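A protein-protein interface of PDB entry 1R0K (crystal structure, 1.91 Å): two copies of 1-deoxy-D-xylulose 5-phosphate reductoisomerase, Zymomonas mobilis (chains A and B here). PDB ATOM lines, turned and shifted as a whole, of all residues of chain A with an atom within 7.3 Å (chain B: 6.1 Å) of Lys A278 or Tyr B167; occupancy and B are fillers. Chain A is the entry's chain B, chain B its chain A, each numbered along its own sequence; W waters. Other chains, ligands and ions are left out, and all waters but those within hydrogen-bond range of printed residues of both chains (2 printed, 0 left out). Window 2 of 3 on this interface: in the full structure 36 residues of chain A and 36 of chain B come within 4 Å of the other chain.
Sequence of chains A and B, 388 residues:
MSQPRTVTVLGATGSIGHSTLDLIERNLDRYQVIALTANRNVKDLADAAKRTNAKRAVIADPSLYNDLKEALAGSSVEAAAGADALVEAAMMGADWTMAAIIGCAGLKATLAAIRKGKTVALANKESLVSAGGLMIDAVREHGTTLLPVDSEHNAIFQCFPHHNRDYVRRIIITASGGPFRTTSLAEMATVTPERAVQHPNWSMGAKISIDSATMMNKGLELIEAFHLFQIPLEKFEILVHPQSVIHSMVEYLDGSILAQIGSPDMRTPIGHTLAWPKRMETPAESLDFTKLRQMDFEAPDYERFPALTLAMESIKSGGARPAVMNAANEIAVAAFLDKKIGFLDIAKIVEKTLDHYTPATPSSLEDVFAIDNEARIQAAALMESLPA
N of Arg A279 lies close to OH of Tyr B167 (3.4 Å). NH2 of Arg B169 is in salt-bridge range of OE2 of Glu A281. OD2 of Asp B254 lies within salt-bridge range of NH1 of Arg A279. The backbone carbonyl oxygen (O) of Met A280 sits close to the backbone NH (N) of Asp B254 (3.4 Å).
Of the 12 printed residues of chain A, 4 touch a printed residue of chain B. Printed residues of chain B that touch a printed residue of chain A: Tyr B167, Arg B169, Tyr B252, Leu B253 and Asp B254. Among the printed residues, 8 pairs touch across the chains.
Water W1 lies within hydrogen-bond range of the side-chain carboxylate (OD2) of Asp B254 (2.6 Å) and the guanidinium group (NH1) of Arg A279 (3.4 Å). Water W2 lies within hydrogen-bond range of the side-chain carboxylate (OD2) of Asp B254, the backbone NH (N) of Met A280 and the backbone carbonyl oxygen (O) of Gly A271.
Lys A278 touches just one residue of chain B: Tyr B167 (3.1 Å). Of the printed residues of chain B, Arg A279 touches Tyr B167, Tyr B252 and Asp B254. Asn B164 touches none of the printed residues of chain A. Of chain A, only Lys A278 and Arg A279 come within 4 Å of Tyr B167. Printed residues of chain A within 4 Å of Asp B254: Arg A279 and Met A280. The nearest residue of chain A that does not touch Tyr B167 is Pro A277 (5.2 Å).
Among the printed residues, merely in contact across the chains: Lys A278 with Tyr B167, Arg A279 with Tyr B252, Met A280 with Leu B253 and Glu A281 with Leu B253.
The backbone carbonyl oxygen of Tyr B167 sits at hydrogen-bond distance from the backbone NH of Leu B253, 2.9 Å away. The side-chain carboxylate (OE2) of Glu B251 lies within salt-bridge range of the guanidinium group (NH1) of Arg B169, at 3.2 Å. The backbone carbonyl oxygen of Leu B253 sits at hydrogen-bond distance from the guanidinium group of Arg B169 (2.7 Å).
No position is printed for both chains.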
ATOM      1  N   ARG A  30       5.519  -3.613  23.203  1.00  0.00           N
ATOM      2  CA  ARG A  30       6.573  -2.620  22.991  1.00  0.00           C
ATOM      3  C   ARG A  30       6.054  -1.363  22.292  1.00  0.00           C
ATOM      4  O   ARG A  30       6.624  -0.280  22.438  1.00  0.00           O
ATOM      5  CB  ARG A  30       7.702  -3.228  22.148  1.00  0.00           C
ATOM      6  CG  ARG A  30       8.569  -4.253  22.876  1.00  0.00           C
ATOM      7  CD  ARG A  30       9.398  -5.088  21.896  1.00  0.00           C
ATOM      8  NE  ARG A  30      10.102  -4.265  20.914  1.00  0.00           N
ATOM      9  CZ  ARG A  30      10.753  -4.746  19.854  1.00  0.00           C
ATOM     10  NH1 ARG A  30      10.798  -6.055  19.629  1.00  0.00           N
ATOM     11  NH2 ARG A  30      11.353  -3.913  19.009  1.00  0.00           N
ATOM     12  N   GLY A 271      11.829  -3.143   9.674  1.00  0.00           N
ATOM     13  CA  GLY A 271      12.256  -3.539  11.006  1.00  0.00           C
ATOM     14  C   GLY A 271      13.441  -2.706  11.468  1.00  0.00           C
ATOM     15  O   GLY A 271      13.570  -2.389  12.649  1.00  0.00           O
ATOM     16  N   HIS A 272      14.318  -2.352  10.534  1.00  0.00           N
ATOM     17  CA  HIS A 272      15.478  -1.538  10.876  1.00  0.00           C
ATOM     18  C   HIS A 272      15.047  -0.141  11.317  1.00  0.00           C
ATOM     19  O   HIS A 272      15.569   0.388  12.297  1.00  0.00           O
ATOM     20  CB  HIS A 272      16.446  -1.444   9.678  1.00  0.00           C
ATOM     21  CG  HIS A 272      17.462  -0.344   9.798  1.00  0.00           C
ATOM     22  ND1 HIS A 272      17.194   0.959   9.437  1.00  0.00           N
ATOM     23  CD2 HIS A 272      18.739  -0.353  10.250  1.00  0.00           C
ATOM     24  CE1 HIS A 272      18.262   1.706   9.661  1.00  0.00           C
ATOM     25  NE2 HIS A 272      19.213   0.934  10.155  1.00  0.00           N
ATOM     26  N   THR A 273      14.092   0.456  10.610  1.00  0.00           N
ATOM     27  CA  THR A 273      13.664   1.803  10.972  1.00  0.00           C
ATOM     28  C   THR A 273      12.826   1.802  12.242  1.00  0.00           C
ATOM     29  O   THR A 273      12.846   2.761  13.009  1.00  0.00           O
ATOM     30  CB  THR A 273      12.854   2.482   9.833  1.00  0.00           C
ATOM     31  OG1 THR A 273      11.589   1.831   9.681  1.00  0.00           O
ATOM     32  CG2 THR A 273      13.618   2.404   8.513  1.00  0.00           C
ATOM     33  N   LEU A 274      12.098   0.712  12.464  1.00  0.00           N
ATOM     34  CA  LEU A 274      11.247   0.593  13.642  1.00  0.00           C
ATOM     35  C   LEU A 274      12.065   0.410  14.925  1.00  0.00           C
ATOM     36  O   LEU A 274      11.782   1.036  15.946  1.00  0.00           O
ATOM     37  CB  LEU A 274      10.259  -0.572  13.456  1.00  0.00           C
ATOM     38  CG  LEU A 274       9.263  -0.799  14.599  1.00  0.00           C
ATOM     39  CD1 LEU A 274       8.471   0.481  14.853  1.00  0.00           C
ATOM     40  CD2 LEU A 274       8.329  -1.955  14.261  1.00  0.00           C
ATOM     41  N   ALA A 275      13.099  -0.423  14.870  1.00  0.00           N
ATOM     42  CA  ALA A 275      13.927  -0.673  16.047  1.00  0.00           C
ATOM     43  C   ALA A 275      15.038   0.358  16.283  1.00  0.00           C
ATOM     44  O   ALA A 275      15.483   0.537  17.418  1.00  0.00           O
ATOM     45  CB  ALA A 275      14.539  -2.071  15.959  1.00  0.00           C
ATOM     46  N   TRP A 276      15.485   1.024  15.219  1.00  0.00           N
ATOM     47  CA  TRP A 276      16.566   2.011  15.323  1.00  0.00           C
ATOM     48  C   TRP A 276      16.447   2.840  16.602  1.00  0.00           C
ATOM     49  O   TRP A 276      15.362   3.312  16.936  1.00  0.00           O
ATOM     50  CB  TRP A 276      16.553   2.950  14.111  1.00  0.00           C
ATOM     51  CG  TRP A 276      17.843   3.687  13.951  1.00  0.00           C
ATOM     52  CD1 TRP A 276      18.967   3.243  13.309  1.00  0.00           C
ATOM     53  CD2 TRP A 276      18.182   4.951  14.527  1.00  0.00           C
ATOM     54  NE1 TRP A 276      19.986   4.152  13.456  1.00  0.00           N
ATOM     55  CE2 TRP A 276      19.533   5.209  14.198  1.00  0.00           C
ATOM     56  CE3 TRP A 276      17.478   5.890  15.293  1.00  0.00           C
ATOM     57  CZ2 TRP A 276      20.194   6.370  14.612  1.00  0.00           C
ATOM     58  CZ3 TRP A 276      18.136   7.046  15.705  1.00  0.00           C
ATOM     59  CH2 TRP A 276      19.482   7.275  15.362  1.00  0.00           C
ATOM     60  N   PRO A 277      17.570   3.061  17.315  1.00  0.00           N
ATOM     61  CA  PRO A 277      18.937   2.612  17.029  1.00  0.00           C
ATOM     62  C   PRO A 277      19.248   1.160  17.397  1.00  0.00           C
ATOM     63  O   PRO A 277      20.393   0.720  17.285  1.00  0.00           O
ATOM     64  CB  PRO A 277      19.784   3.600  17.824  1.00  0.00           C
ATOM     65  CG  PRO A 277      18.955   3.794  19.054  1.00  0.00           C
ATOM     66  CD  PRO A 277      17.558   3.963  18.483  1.00  0.00           C
ATOM     67  N   LYS A 278      18.236   0.423  17.843  1.00  0.00           N
ATOM     68  CA  LYS A 278      18.419  -0.978  18.206  1.00  0.00           C
ATOM     69  C   LYS A 278      18.045  -1.842  17.007  1.00  0.00           C
ATOM     70  O   LYS A 278      17.774  -1.330  15.921  1.00  0.00           O
ATOM     71  CB  LYS A 278      17.516  -1.341  19.389  1.00  0.00           C
ATOM     72  CG  LYS A 278      17.711  -0.468  20.612  1.00  0.00           C
ATOM     73  CD  LYS A 278      16.738  -0.862  21.714  1.00  0.00           C
ATOM     74  CE  LYS A 278      16.971  -0.044  22.977  1.00  0.00           C
ATOM     75  NZ  LYS A 278      16.025  -0.430  24.062  1.00  0.00           N
ATOM     76  N   ARG A 279      18.035  -3.155  17.208  1.00  0.00           N
ATOM     77  CA  ARG A 279      17.659  -4.088  16.155  1.00  0.00           C
ATOM     78  C   ARG A 279      16.568  -4.983  16.728  1.00  0.00           C
ATOM     79  O   ARG A 279      16.539  -5.243  17.935  1.00  0.00           O
ATOM     80  CB  ARG A 279      18.852  -4.951  15.731  1.00  0.00           C
ATOM     81  CG  ARG A 279      19.953  -4.203  14.998  1.00  0.00           C
ATOM     82  CD  ARG A 279      19.656  -4.060  13.514  1.00  0.00           C
ATOM     83  NE  ARG A 279      20.773  -3.428  12.809  1.00  0.00           N
ATOM     84  CZ  ARG A 279      20.911  -3.404  11.486  1.00  0.00           C
ATOM     85  NH1 ARG A 279      20.001  -3.975  10.704  1.00  0.00           N
ATOM     86  NH2 ARG A 279      21.968  -2.811  10.941  1.00  0.00           N
ATOM     87  N   MET A 280      15.664  -5.436  15.872  1.00  0.00           N
ATOM     88  CA  MET A 280      14.587  -6.311  16.313  1.00  0.00           C
ATOM     89  C   MET A 280      14.512  -7.496  15.374  1.00  0.00           C
ATOM     90  O   MET A 280      14.934  -7.420  14.224  1.00  0.00           O
ATOM     91  CB  MET A 280      13.246  -5.577  16.285  1.00  0.00           C
ATOM     92  CG  MET A 280      12.749  -5.265  14.883  1.00  0.00           C
ATOM     93  SD  MET A 280      11.272  -4.223  14.871  1.00  0.00           S
ATOM     94  CE  MET A 280       9.997  -5.412  15.358  1.00  0.00           C
ATOM     95  N   GLU A 281      13.971  -8.599  15.862  1.00  0.00           N
ATOM     96  CA  GLU A 281      13.841  -9.758  15.011  1.00  0.00           C
ATOM     97  C   GLU A 281      12.628  -9.565  14.100  1.00  0.00           C
ATOM     98  O   GLU A 281      11.673  -8.873  14.461  1.00  0.00           O
ATOM     99  CB  GLU A 281      13.664 -11.016  15.862  1.00  0.00           C
ATOM    100  CG  GLU A 281      13.551 -12.284  15.040  1.00  0.00           C
ATOM    101  CD  GLU A 281      13.791 -13.527  15.858  1.00  0.00           C
ATOM    102  OE1 GLU A 281      13.097 -13.708  16.880  1.00  0.00           O
ATOM    103  OE2 GLU A 281      14.677 -14.324  15.477  1.00  0.00           O
ATOM    104  N   PRO B 161      27.752  -5.911  15.350  1.00  0.00           N
ATOM    105  CA  PRO B 161      27.124  -5.006  16.315  1.00  0.00           C
ATOM    106  C   PRO B 161      27.823  -5.132  17.666  1.00  0.00           C
ATOM    107  O   PRO B 161      27.415  -5.922  18.519  1.00  0.00           O
ATOM    108  CB  PRO B 161      25.685  -5.506  16.359  1.00  0.00           C
ATOM    109  CG  PRO B 161      25.874  -6.989  16.248  1.00  0.00           C
ATOM    110  CD  PRO B 161      26.918  -7.109  15.140  1.00  0.00           C
ATOM    111  N   ASN B 164      26.253  -5.525  21.321  1.00  0.00           N
ATOM    112  CA  ASN B 164      24.938  -6.121  21.102  1.00  0.00           C
ATOM    113  C   ASN B 164      25.104  -7.410  20.311  1.00  0.00           C
ATOM    114  O   ASN B 164      24.564  -7.548  19.213  1.00  0.00           O
ATOM    115  CB  ASN B 164      24.027  -5.159  20.331  1.00  0.00           C
ATOM    116  CG  ASN B 164      23.593  -3.972  21.165  1.00  0.00           C
ATOM    117  OD1 ASN B 164      22.853  -4.119  22.137  1.00  0.00           O
ATOM    118  ND2 ASN B 164      24.056  -2.785  20.790  1.00  0.00           N
ATOM    119  N   ARG B 165      25.859  -8.347  20.878  1.00  0.00           N
ATOM    120  CA  ARG B 165      26.123  -9.631  20.234  1.00  0.00           C
ATOM    121  C   ARG B 165      24.843 -10.404  19.945  1.00  0.00           C
ATOM    122  O   ARG B 165      24.783 -11.176  18.988  1.00  0.00           O
ATOM    123  CB  ARG B 165      27.029 -10.492  21.114  1.00  0.00           C
ATOM    124  CG  ARG B 165      28.327  -9.822  21.527  1.00  0.00           C
ATOM    125  CD  ARG B 165      29.273 -10.836  22.162  1.00  0.00           C
ATOM    126  NE  ARG B 165      28.638 -11.568  23.253  1.00  0.00           N
ATOM    127  CZ  ARG B 165      28.285 -11.028  24.414  1.00  0.00           C
ATOM    128  NH1 ARG B 165      28.508  -9.740  24.644  1.00  0.00           N
ATOM    129  NH2 ARG B 165      27.705 -11.774  25.345  1.00  0.00           N
ATOM    130  N   ASP B 166      23.826 -10.199  20.774  1.00  0.00           N
ATOM    131  CA  ASP B 166      22.549 -10.885  20.611  1.00  0.00           C
ATOM    132  C   ASP B 166      21.818 -10.513  19.326  1.00  0.00           C
ATOM    133  O   ASP B 166      20.837 -11.158  18.958  1.00  0.00           O
ATOM    134  CB  ASP B 166      21.662 -10.596  21.823  1.00  0.00           C
ATOM    135  CG  ASP B 166      22.243 -11.153  23.105  1.00  0.00           C
ATOM    136  OD1 ASP B 166      23.429 -11.552  23.089  1.00  0.00           O
ATOM    137  OD2 ASP B 166      21.525 -11.191  24.130  1.00  0.00           O
ATOM    138  N   TYR B 167      22.290  -9.476  18.645  1.00  0.00           N
ATOM    139  CA  TYR B 167      21.670  -9.056  17.397  1.00  0.00           C
ATOM    140  C   TYR B 167      22.113  -9.946  16.234  1.00  0.00           C
ATOM    141  O   TYR B 167      21.470  -9.976  15.182  1.00  0.00           O
ATOM    142  CB  TYR B 167      22.046  -7.610  17.062  1.00  0.00           C
ATOM    143  CG  TYR B 167      21.396  -6.546  17.912  1.00  0.00           C
ATOM    144  CD1 TYR B 167      20.371  -6.855  18.817  1.00  0.00           C
ATOM    145  CD2 TYR B 167      21.792  -5.216  17.796  1.00  0.00           C
ATOM    146  CE1 TYR B 167      19.764  -5.859  19.581  1.00  0.00           C
ATOM    147  CE2 TYR B 167      21.193  -4.215  18.549  1.00  0.00           C
ATOM    148  CZ  TYR B 167      20.182  -4.540  19.442  1.00  0.00           C
ATOM    149  OH  TYR B 167      19.609  -3.543  20.198  1.00  0.00           O
ATOM    150  N   VAL B 168      23.212 -10.668  16.417  1.00  0.00           N
ATOM    151  CA  VAL B 168      23.731 -11.522  15.351  1.00  0.00           C
ATOM    152  C   VAL B 168      23.011 -12.859  15.230  1.00  0.00           C
ATOM    153  O   VAL B 168      22.827 -13.569  16.217  1.00  0.00           O
ATOM    154  CB  VAL B 168      25.241 -11.805  15.550  1.00  0.00           C
ATOM    155  CG1 VAL B 168      25.770 -12.654  14.399  1.00  0.00           C
ATOM    156  CG2 VAL B 168      26.008 -10.488  15.638  1.00  0.00           C
ATOM    157  N   ARG B 169      22.601 -13.198  14.011  1.00  0.00           N
ATOM    158  CA  ARG B 169      21.937 -14.472  13.754  1.00  0.00           C
ATOM    159  C   ARG B 169      22.980 -15.465  13.252  1.00  0.00           C
ATOM    160  O   ARG B 169      22.926 -16.659  13.561  1.00  0.00           O
ATOM    161  CB  ARG B 169      20.828 -14.311  12.707  1.00  0.00           C
ATOM    162  CG  ARG B 169      20.235 -15.643  12.243  1.00  0.00           C
ATOM    163  CD  ARG B 169      18.969 -15.427  11.434  1.00  0.00           C
ATOM    164  NE  ARG B 169      17.886 -14.916  12.270  1.00  0.00           N
ATOM    165  CZ  ARG B 169      16.993 -14.021  11.868  1.00  0.00           C
ATOM    166  NH1 ARG B 169      17.057 -13.529  10.635  1.00  0.00           N
ATOM    167  NH2 ARG B 169      16.036 -13.624  12.697  1.00  0.00           N
ATOM    168  N   LYS B 235      26.567 -20.446  15.247  1.00  0.00           N
ATOM    169  CA  LYS B 235      26.172 -19.280  14.465  1.00  0.00           C
ATOM    170  C   LYS B 235      27.170 -18.958  13.349  1.00  0.00           C
ATOM    171  O   LYS B 235      26.918 -18.083  12.519  1.00  0.00           O
ATOM    172  CB  LYS B 235      25.987 -18.059  15.375  1.00  0.00           C
ATOM    173  CG  LYS B 235      24.729 -18.123  16.247  1.00  0.00           C
ATOM    174  CD  LYS B 235      24.458 -16.803  16.948  1.00  0.00           C
ATOM    175  CE  LYS B 235      23.149 -16.847  17.728  1.00  0.00           C
ATOM    176  NZ  LYS B 235      22.854 -15.538  18.383  1.00  0.00           N
ATOM    177  N   GLU B 251      24.831 -11.481   9.626  1.00  0.00           N
ATOM    178  CA  GLU B 251      23.386 -11.346   9.458  1.00  0.00           C
ATOM    179  C   GLU B 251      22.770 -10.989  10.791  1.00  0.00           C
ATOM    180  O   GLU B 251      23.087 -11.593  11.815  1.00  0.00           O
ATOM    181  CB  GLU B 251      22.736 -12.637   8.959  1.00  0.00           C
ATOM    182  CG  GLU B 251      21.281 -12.410   8.528  1.00  0.00           C
ATOM    183  CD  GLU B 251      20.545 -13.691   8.183  1.00  0.00           C
ATOM    184  OE1 GLU B 251      21.177 -14.600   7.614  1.00  0.00           O
ATOM    185  OE2 GLU B 251      19.328 -13.784   8.464  1.00  0.00           O
ATOM    186  N   TYR B 252      21.876 -10.006  10.769  1.00  0.00           N
ATOM    187  CA  TYR B 252      21.209  -9.552  11.974  1.00  0.00           C
ATOM    188  C   TYR B 252      19.843 -10.212  12.105  1.00  0.00           C
ATOM    189  O   TYR B 252      19.313 -10.763  11.136  1.00  0.00           O
ATOM    190  CB  TYR B 252      21.057  -8.028  11.948  1.00  0.00           C
ATOM    191  CG  TYR B 252      22.362  -7.283  12.110  1.00  0.00           C
ATOM    192  CD1 TYR B 252      23.388  -7.415  11.173  1.00  0.00           C
ATOM    193  CD2 TYR B 252      22.584  -6.468  13.216  1.00  0.00           C
ATOM    194  CE1 TYR B 252      24.611  -6.750  11.341  1.00  0.00           C
ATOM    195  CE2 TYR B 252      23.798  -5.800  13.392  1.00  0.00           C
ATOM    196  CZ  TYR B 252      24.803  -5.946  12.455  1.00  0.00           C
ATOM    197  OH  TYR B 252      25.997  -5.287  12.639  1.00  0.00           O
ATOM    198  N   LEU B 253      19.286 -10.149  13.310  1.00  0.00           N
ATOM    199  CA  LEU B 253      17.988 -10.738  13.614  1.00  0.00           C
ATOM    200  C   LEU B 253      16.863 -10.256  12.710  1.00  0.00           C
ATOM    201  O   LEU B 253      15.857 -10.946  12.554  1.00  0.00           O
ATOM    202  CB  LEU B 253      17.600 -10.444  15.066  1.00  0.00           C
ATOM    203  CG  LEU B 253      18.547 -10.918  16.169  1.00  0.00           C
ATOM    204  CD1 LEU B 253      17.907 -10.636  17.527  1.00  0.00           C
ATOM    205  CD2 LEU B 253      18.829 -12.403  16.005  1.00  0.00           C
ATOM    206  N   ASP B 254      17.017  -9.073  12.123  1.00  0.00           N
ATOM    207  CA  ASP B 254      15.971  -8.559  11.253  1.00  0.00           C
ATOM    208  C   ASP B 254      16.094  -9.051   9.817  1.00  0.00           C
ATOM    209  O   ASP B 254      15.280  -8.695   8.964  1.00  0.00           O
ATOM    210  CB  ASP B 254      15.930  -7.025  11.282  1.00  0.00           C
ATOM    211  CG  ASP B 254      17.263  -6.389  10.927  1.00  0.00           C
ATOM    212  OD1 ASP B 254      18.154  -7.104  10.422  1.00  0.00           O
ATOM    213  OD2 ASP B 254      17.407  -5.167  11.155  1.00  0.00           O
HETATM  214  O   HOH W   1      17.285  -4.311   8.732  1.00  0.00           O
HETATM  215  O   HOH W   2      16.048  -4.144  13.391  1.00  0.00           O
